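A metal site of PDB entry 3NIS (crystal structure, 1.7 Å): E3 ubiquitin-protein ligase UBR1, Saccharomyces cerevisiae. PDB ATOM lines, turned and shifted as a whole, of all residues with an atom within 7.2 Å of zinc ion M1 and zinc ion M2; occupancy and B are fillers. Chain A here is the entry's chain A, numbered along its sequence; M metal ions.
The backbone carbonyl oxygen (O) of Cys 65 sits at hydrogen-bond distance from the backbone NH (N) of Cys 11 (2.7 Å).
The side-chain sulfur of Cys 63 sits close to the backbone NH of Cys 65, 3.4 Å away.
SG of Cys 77 sits close to N of Ala 79.
The backbone NH (N) of Arg 13 lies close to the side-chain sulfur (SG) of Cys 11.
O of Cys 11 is in hydrogen-bond range of NH2 of Arg 9 (3.0 Å).
N of Cys 63 sits at hydrogen-bond distance from O of Arg 13, 2.9 Å away.
The backbone carbonyl oxygen (O) of Cys 63 lies within hydrogen-bond range of the backbone NH (N) of Gly 12 (2.9 Å).
The backbone carbonyl oxygen (O) of Cys 39 lies within hydrogen-bond range of the backbone NH (N) of Lys 78 (3.0 Å).
The nearest printed residue that does not touch zinc ion M1 is Cys 11 (4.4 Å).
Within 4 Å of zinc ion M2: Cys 11, Cys 36, Cys 39 and Cys 63.
The nearest printed residue that does not touch zinc ion M2 is Cys 65 (4.2 Å).
NE2 of His 6 binds zinc ion M1, 2.1 Å away.
Zinc ion M1 is bound by SG of Cys 65 (2.3 Å).
Zinc ion M1 is bound by SG of Cys 77.
Zinc ion M1 is bound by SG of Cys 39 (2.4 Å).
Zinc ion M1 has four donor atoms within binding distance.
Zinc ion M2 is bound by SG of Cys 11 (2.3 Å), SG of Cys 63 (2.3 Å), SG of Cys 36 (2.4 Å) and SG of Cys 39 (2.4 Å).
Zinc ion M2 has four donor atoms within binding distance.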
ATOM      1  N   HIS A   4       0.667  14.701 -15.345  1.00  0.00           N
ATOM      2  CA  HIS A   4       1.807  15.364 -15.947  1.00  0.00           C
ATOM      3  C   HIS A   4       3.036  14.834 -15.234  1.00  0.00           C
ATOM      4  O   HIS A   4       3.269  15.142 -14.062  1.00  0.00           O
ATOM      5  CB  HIS A   4       1.704  16.885 -15.824  1.00  0.00           C
ATOM      6  CG  HIS A   4       2.483  17.628 -16.872  1.00  0.00           C
ATOM      7  ND1 HIS A   4       3.856  17.565 -16.966  1.00  0.00           N
ATOM      8  CD2 HIS A   4       2.076  18.468 -17.849  1.00  0.00           C
ATOM      9  CE1 HIS A   4       4.255  18.332 -17.970  1.00  0.00           C
ATOM     10  NE2 HIS A   4       3.197  18.891 -18.520  1.00  0.00           N
ATOM     11  N   LYS A   5       3.785  14.001 -15.937  1.00  0.00           N
ATOM     12  CA  LYS A   5       4.934  13.333 -15.355  1.00  0.00           C
ATOM     13  C   LYS A   5       6.112  14.271 -15.322  1.00  0.00           C
ATOM     14  O   LYS A   5       6.217  15.190 -16.163  1.00  0.00           O
ATOM     15  CB  LYS A   5       5.280  12.088 -16.175  1.00  0.00           C
ATOM     16  CG  LYS A   5       4.108  11.146 -16.358  1.00  0.00           C
ATOM     17  CD  LYS A   5       4.465  10.034 -17.306  1.00  0.00           C
ATOM     18  CE  LYS A   5       3.269   9.142 -17.548  1.00  0.00           C
ATOM     19  NZ  LYS A   5       3.665   7.960 -18.368  1.00  0.00           N
ATOM     20  N   HIS A   6       7.004  14.047 -14.362  1.00  0.00           N
ATOM     21  CA  HIS A   6       8.257  14.790 -14.288  1.00  0.00           C
ATOM     22  C   HIS A   6       9.446  13.842 -14.476  1.00  0.00           C
ATOM     23  O   HIS A   6      10.477  13.981 -13.827  1.00  0.00           O
ATOM     24  CB  HIS A   6       8.359  15.537 -12.966  1.00  0.00           C
ATOM     25  CG  HIS A   6       8.289  14.655 -11.766  1.00  0.00           C
ATOM     26  ND1 HIS A   6       9.410  14.025 -11.250  1.00  0.00           N
ATOM     27  CD2 HIS A   6       7.251  14.286 -10.980  1.00  0.00           C
ATOM     28  CE1 HIS A   6       9.049  13.303 -10.197  1.00  0.00           C
ATOM     29  NE2 HIS A   6       7.749  13.446 -10.014  1.00  0.00           N
ATOM     30  N   ARG A   9      13.576  13.991 -13.741  1.00  0.00           N
ATOM     31  CA  ARG A   9      13.846  15.107 -12.847  1.00  0.00           C
ATOM     32  C   ARG A   9      12.974  15.046 -11.604  1.00  0.00           C
ATOM     33  O   ARG A   9      12.142  14.131 -11.453  1.00  0.00           O
ATOM     34  CB  ARG A   9      13.683  16.461 -13.558  1.00  0.00           C
ATOM     35  CG  ARG A   9      12.348  16.643 -14.280  1.00  0.00           C
ATOM     36  CD  ARG A   9      12.019  18.098 -14.445  1.00  0.00           C
ATOM     37  NE  ARG A   9      11.514  18.697 -13.201  1.00  0.00           N
ATOM     38  CZ  ARG A   9      10.988  19.911 -13.125  1.00  0.00           C
ATOM     39  NH1 ARG A   9      10.923  20.690 -14.209  1.00  0.00           N
ATOM     40  NH2 ARG A   9      10.531  20.368 -11.972  1.00  0.00           N
ATOM     41  N   ASN A  10      13.183  15.993 -10.698  1.00  0.00           N
ATOM     42  CA  ASN A  10      12.374  16.119  -9.497  1.00  0.00           C
ATOM     43  C   ASN A  10      11.004  16.717  -9.831  1.00  0.00           C
ATOM     44  O   ASN A  10      10.827  17.336 -10.885  1.00  0.00           O
ATOM     45  CB  ASN A  10      13.070  17.041  -8.498  1.00  0.00           C
ATOM     46  CG  ASN A  10      13.137  18.474  -9.000  1.00  0.00           C
ATOM     47  OD1 ASN A  10      13.638  18.730 -10.091  1.00  0.00           O
ATOM     48  ND2 ASN A  10      12.612  19.413  -8.214  1.00  0.00           N
ATOM     49  N   CYS A  11      10.056  16.560  -8.916  1.00  0.00           N
ATOM     50  CA  CYS A  11       8.749  17.205  -9.059  1.00  0.00           C
ATOM     51  C   CYS A  11       8.861  18.720  -8.805  1.00  0.00           C
ATOM     52  O   CYS A  11       8.723  19.528  -9.739  1.00  0.00           O
ATOM     53  CB  CYS A  11       7.721  16.563  -8.132  1.00  0.00           C
ATOM     54  SG  CYS A  11       6.122  17.395  -8.172  1.00  0.00           S
ATOM     55  N   GLY A  12       9.141  19.080  -7.555  1.00  0.00           N
ATOM     56  CA  GLY A  12       9.339  20.486  -7.169  1.00  0.00           C
ATOM     57  C   GLY A  12       8.088  21.348  -7.248  1.00  0.00           C
ATOM     58  O   GLY A  12       8.175  22.580  -7.171  1.00  0.00           O
ATOM     59  N   ARG A  13       6.933  20.714  -7.403  1.00  0.00           N
ATOM     60  CA  ARG A  13       5.652  21.427  -7.458  1.00  0.00           C
ATOM     61  C   ARG A  13       5.355  22.138  -6.136  1.00  0.00           C
ATOM     62  O   ARG A  13       5.427  21.535  -5.067  1.00  0.00           O
ATOM     63  CB  ARG A  13       4.528  20.430  -7.780  1.00  0.00           C
ATOM     64  CG  ARG A  13       3.123  21.002  -7.889  1.00  0.00           C
ATOM     65  CD  ARG A  13       2.140  19.856  -8.189  1.00  0.00           C
ATOM     66  NE  ARG A  13       0.734  20.252  -8.200  1.00  0.00           N
ATOM     67  CZ  ARG A  13      -0.049  20.331  -7.113  1.00  0.00           C
ATOM     68  NH1 ARG A  13       0.446  20.055  -5.906  1.00  0.00           N
ATOM     69  NH2 ARG A  13      -1.320  20.696  -7.240  1.00  0.00           N
ATOM     70  N   PHE A  15       2.939  23.504  -3.380  1.00  0.00           N
ATOM     71  CA  PHE A  15       1.643  23.037  -2.901  1.00  0.00           C
ATOM     72  C   PHE A  15       0.579  24.115  -3.048  1.00  0.00           C
ATOM     73  O   PHE A  15       0.857  25.304  -2.937  1.00  0.00           O
ATOM     74  CB  PHE A  15       1.745  22.587  -1.452  1.00  0.00           C
ATOM     75  CG  PHE A  15       2.545  21.343  -1.283  1.00  0.00           C
ATOM     76  CD1 PHE A  15       1.972  20.092  -1.479  1.00  0.00           C
ATOM     77  CD2 PHE A  15       3.891  21.413  -0.942  1.00  0.00           C
ATOM     78  CE1 PHE A  15       2.716  18.935  -1.334  1.00  0.00           C
ATOM     79  CE2 PHE A  15       4.651  20.250  -0.793  1.00  0.00           C
ATOM     80  CZ  PHE A  15       4.057  19.015  -0.980  1.00  0.00           C
ATOM     81  N   VAL A  34       8.657  15.841   1.761  1.00  0.00           N
ATOM     82  CA  VAL A  34       7.216  15.766   1.495  1.00  0.00           C
ATOM     83  C   VAL A  34       6.905  15.418   0.043  1.00  0.00           C
ATOM     84  O   VAL A  34       7.736  15.610  -0.855  1.00  0.00           O
ATOM     85  CB  VAL A  34       6.486  17.069   1.901  1.00  0.00           C
ATOM     86  CG1 VAL A  34       6.515  17.260   3.420  1.00  0.00           C
ATOM     87  CG2 VAL A  34       7.088  18.287   1.158  1.00  0.00           C
ATOM     88  N   LEU A  35       5.703  14.912  -0.165  1.00  0.00           N
ATOM     89  CA  LEU A  35       5.238  14.489  -1.485  1.00  0.00           C
ATOM     90  C   LEU A  35       3.870  15.085  -1.746  1.00  0.00           C
ATOM     91  O   LEU A  35       3.064  15.202  -0.825  1.00  0.00           O
ATOM     92  CB  LEU A  35       5.129  12.964  -1.542  1.00  0.00           C
ATOM     93  CG  LEU A  35       6.433  12.173  -1.493  1.00  0.00           C
ATOM     94  CD1 LEU A  35       6.148  10.692  -1.227  1.00  0.00           C
ATOM     95  CD2 LEU A  35       7.238  12.360  -2.763  1.00  0.00           C
ATOM     96  N   CYS A  36       3.613  15.446  -2.997  1.00  0.00           N
ATOM     97  CA  CYS A  36       2.354  16.043  -3.402  1.00  0.00           C
ATOM     98  C   CYS A  36       1.356  14.971  -3.847  1.00  0.00           C
ATOM     99  O   CYS A  36       1.717  13.790  -4.009  1.00  0.00           O
ATOM    100  CB  CYS A  36       2.571  17.052  -4.536  1.00  0.00           C
ATOM    101  SG  CYS A  36       2.748  16.318  -6.178  1.00  0.00           S
ATOM    102  N   ILE A  37       0.124  15.397  -4.077  1.00  0.00           N
ATOM    103  CA  ILE A  37      -0.964  14.476  -4.455  1.00  0.00           C
ATOM    104  C   ILE A  37      -0.749  13.783  -5.802  1.00  0.00           C
ATOM    105  O   ILE A  37      -1.274  12.694  -6.049  1.00  0.00           O
ATOM    106  CB  ILE A  37      -2.341  15.170  -4.456  1.00  0.00           C
ATOM    107  CG1 ILE A  37      -2.271  16.478  -5.269  1.00  0.00           C
ATOM    108  CG2 ILE A  37      -2.804  15.436  -3.040  1.00  0.00           C
ATOM    109  CD1 ILE A  37      -3.536  16.852  -6.002  1.00  0.00           C
ATOM    110  N   HIS A  38       0.014  14.437  -6.682  1.00  0.00           N
ATOM    111  CA  HIS A  38       0.330  13.906  -8.004  1.00  0.00           C
ATOM    112  C   HIS A  38       1.323  12.744  -7.909  1.00  0.00           C
ATOM    113  O   HIS A  38       1.348  11.869  -8.779  1.00  0.00           O
ATOM    114  CB  HIS A  38       0.966  14.984  -8.891  1.00  0.00           C
ATOM    115  CG  HIS A  38       0.077  16.138  -9.210  1.00  0.00           C
ATOM    116  ND1 HIS A  38      -1.141  16.346  -8.609  1.00  0.00           N
ATOM    117  CD2 HIS A  38       0.244  17.174 -10.074  1.00  0.00           C
ATOM    118  CE1 HIS A  38      -1.693  17.442  -9.095  1.00  0.00           C
ATOM    119  NE2 HIS A  38      -0.877  17.962  -9.985  1.00  0.00           N
ATOM    120  N   CYS A  39       2.110  12.722  -6.838  1.00  0.00           N
ATOM    121  CA  CYS A  39       3.294  11.876  -6.744  1.00  0.00           C
ATOM    122  C   CYS A  39       3.187  10.770  -5.705  1.00  0.00           C
ATOM    123  O   CYS A  39       3.695   9.652  -5.906  1.00  0.00           O
ATOM    124  CB  CYS A  39       4.501  12.740  -6.405  1.00  0.00           C
ATOM    125  SG  CYS A  39       4.988  13.835  -7.749  1.00  0.00           S
ATOM    126  N   PHE A  40       2.563  11.089  -4.578  1.00  0.00           N
ATOM    127  CA  PHE A  40       2.433  10.127  -3.501  1.00  0.00           C
ATOM    128  C   PHE A  40       1.766   8.843  -3.982  1.00  0.00           C
ATOM    129  O   PHE A  40       0.639   8.873  -4.480  1.00  0.00           O
ATOM    130  CB  PHE A  40       1.661  10.736  -2.320  1.00  0.00           C
ATOM    131  CG  PHE A  40       1.488   9.780  -1.180  1.00  0.00           C
ATOM    132  CD1 PHE A  40       2.499   9.616  -0.228  1.00  0.00           C
ATOM    133  CD2 PHE A  40       0.315   9.016  -1.056  1.00  0.00           C
ATOM    134  CE1 PHE A  40       2.343   8.747   0.816  1.00  0.00           C
ATOM    135  CE2 PHE A  40       0.148   8.125   0.002  1.00  0.00           C
ATOM    136  CZ  PHE A  40       1.171   7.983   0.940  1.00  0.00           C
ATOM    137  N   ILE A  62       7.569  22.682  -1.461  1.00  0.00           N
ATOM    138  CA  ILE A  62       7.622  22.037  -2.765  1.00  0.00           C
ATOM    139  C   ILE A  62       7.773  20.515  -2.625  1.00  0.00           C
ATOM    140  O   ILE A  62       8.387  20.024  -1.670  1.00  0.00           O
ATOM    141  CB  ILE A  62       8.753  22.635  -3.661  1.00  0.00           C
ATOM    142  CG1 ILE A  62      10.142  22.456  -3.037  1.00  0.00           C
ATOM    143  CG2 ILE A  62       8.479  24.098  -3.974  1.00  0.00           C
ATOM    144  CD1 ILE A  62      10.927  21.244  -3.588  1.00  0.00           C
ATOM    145  N   CYS A  63       7.217  19.787  -3.585  1.00  0.00           N
ATOM    146  CA  CYS A  63       7.286  18.334  -3.581  1.00  0.00           C
ATOM    147  C   CYS A  63       8.692  17.812  -3.866  1.00  0.00           C
ATOM    148  O   CYS A  63       9.365  18.274  -4.782  1.00  0.00           O
ATOM    149  CB  CYS A  63       6.310  17.793  -4.623  1.00  0.00           C
ATOM    150  SG  CYS A  63       6.358  16.027  -4.779  1.00  0.00           S
ATOM    151  N   ASP A  64       9.137  16.839  -3.062  1.00  0.00           N
ATOM    152  CA  ASP A  64      10.479  16.299  -3.178  1.00  0.00           C
ATOM    153  C   ASP A  64      10.575  15.003  -3.980  1.00  0.00           C
ATOM    154  O   ASP A  64      11.638  14.371  -4.025  1.00  0.00           O
ATOM    155  CB  ASP A  64      11.096  16.052  -1.789  1.00  0.00           C
ATOM    156  CG  ASP A  64      11.226  17.301  -0.974  1.00  0.00           C
ATOM    157  OD1 ASP A  64      11.778  18.316  -1.484  1.00  0.00           O
ATOM    158  OD2 ASP A  64      10.765  17.270   0.177  1.00  0.00           O
ATOM    159  N   CYS A  65       9.469  14.600  -4.608  1.00  0.00           N
ATOM    160  CA  CYS A  65       9.485  13.396  -5.431  1.00  0.00           C
ATOM    161  C   CYS A  65      10.553  13.502  -6.522  1.00  0.00           C
ATOM    162  O   CYS A  65      10.621  14.498  -7.237  1.00  0.00           O
ATOM    163  CB  CYS A  65       8.114  13.175  -6.058  1.00  0.00           C
ATOM    164  SG  CYS A  65       7.977  11.652  -7.003  1.00  0.00           S
ATOM    165  N   GLY A  66      11.403  12.489  -6.631  1.00  0.00           N
ATOM    166  CA  GLY A  66      12.476  12.504  -7.613  1.00  0.00           C
ATOM    167  C   GLY A  66      13.732  13.225  -7.169  1.00  0.00           C
ATOM    168  O   GLY A  66      14.697  13.299  -7.938  1.00  0.00           O
ATOM    169  N   LEU A  75      11.301   5.677  -4.721  1.00  0.00           N
ATOM    170  CA  LEU A  75       9.884   6.006  -4.854  1.00  0.00           C
ATOM    171  C   LEU A  75       9.392   5.651  -6.248  1.00  0.00           C
ATOM    172  O   LEU A  75      10.140   5.732  -7.221  1.00  0.00           O
ATOM    173  CB  LEU A  75       9.609   7.492  -4.561  1.00  0.00           C
ATOM    174  CG  LEU A  75       9.915   8.079  -3.181  1.00  0.00           C
ATOM    175  CD1 LEU A  75       9.356   9.475  -3.071  1.00  0.00           C
ATOM    176  CD2 LEU A  75       9.362   7.214  -2.052  1.00  0.00           C
ATOM    177  N   HIS A  76       8.122   5.255  -6.331  1.00  0.00           N
ATOM    178  CA  HIS A  76       7.501   4.982  -7.627  1.00  0.00           C
ATOM    179  C   HIS A  76       6.401   6.013  -7.837  1.00  0.00           C
ATOM    180  O   HIS A  76       5.263   5.837  -7.429  1.00  0.00           O
ATOM    181  CB  HIS A  76       6.982   3.533  -7.670  1.00  0.00           C
ATOM    182  CG  HIS A  76       8.055   2.524  -7.387  1.00  0.00           C
ATOM    183  ND1 HIS A  76       8.333   2.089  -6.106  1.00  0.00           N
ATOM    184  CD2 HIS A  76       8.943   1.921  -8.206  1.00  0.00           C
ATOM    185  CE1 HIS A  76       9.334   1.223  -6.157  1.00  0.00           C
ATOM    186  NE2 HIS A  76       9.721   1.101  -7.416  1.00  0.00           N
ATOM    187  N   CYS A  77       6.797   7.123  -8.442  1.00  0.00           N
ATOM    188  CA  CYS A  77       5.930   8.266  -8.625  1.00  0.00           C
ATOM    189  C   CYS A  77       4.587   7.811  -9.182  1.00  0.00           C
ATOM    190  O   CYS A  77       4.544   7.122 -10.192  1.00  0.00           O
ATOM    191  CB  CYS A  77       6.563   9.285  -9.567  1.00  0.00           C
ATOM    192  SG  CYS A  77       5.523  10.717  -9.839  1.00  0.00           S
ATOM    193  N   LYS A  78       3.507   8.206  -8.513  1.00  0.00           N
ATOM    194  CA  LYS A  78       2.162   7.815  -8.952  1.00  0.00           C
ATOM    195  C   LYS A  78       1.869   8.250 -10.395  1.00  0.00           C
ATOM    196  O   LYS A  78       1.221   7.532 -11.150  1.00  0.00           O
ATOM    197  CB  LYS A  78       1.102   8.372  -7.985  1.00  0.00           C
ATOM    198  CG  LYS A  78      -0.304   7.812  -8.216  1.00  0.00           C
ATOM    199  CD  LYS A  78      -1.192   8.094  -7.018  1.00  0.00           C
ATOM    200  CE  LYS A  78      -2.531   7.376  -7.140  1.00  0.00           C
ATOM    201  NZ  LYS A  78      -3.423   8.089  -8.084  1.00  0.00           N
ATOM    202  N   ALA A  79       2.380   9.422 -10.785  1.00  0.00           N
ATOM    203  CA  ALA A  79       2.180   9.952 -12.142  1.00  0.00           C
ATOM    204  C   ALA A  79       2.697   9.000 -13.225  1.00  0.00           C
ATOM    205  O   ALA A  79       2.161   8.966 -14.322  1.00  0.00           O
ATOM    206  CB  ALA A  79       2.808  11.336 -12.275  1.00  0.00           C
ATOM    207  N   GLU A  80       3.737   8.235 -12.913  1.00  0.00           N
ATOM    208  CA  GLU A  80       4.361   7.332 -13.883  1.00  0.00           C
ATOM    209  C   GLU A  80       3.497   6.116 -14.242  1.00  0.00           C
ATOM    210  O   GLU A  80       3.721   5.470 -15.265  1.00  0.00           O
ATOM    211  CB  GLU A  80       5.748   6.899 -13.397  1.00  0.00           C
ATOM    212  CG  GLU A  80       6.768   8.040 -13.327  1.00  0.00           C
ATOM    213  CD  GLU A  80       7.167   8.583 -14.687  1.00  0.00           C
ATOM    214  OE1 GLU A  80       7.202   7.803 -15.661  1.00  0.00           O
ATOM    215  OE2 GLU A  80       7.456   9.794 -14.785  1.00  0.00           O
HETATM  216 ZN    ZN M   1       6.596  12.363  -8.668  1.00  0.00          ZN
HETATM  217 ZN    ZN M   2       5.060  15.987  -6.687  1.00  0.00          ZN
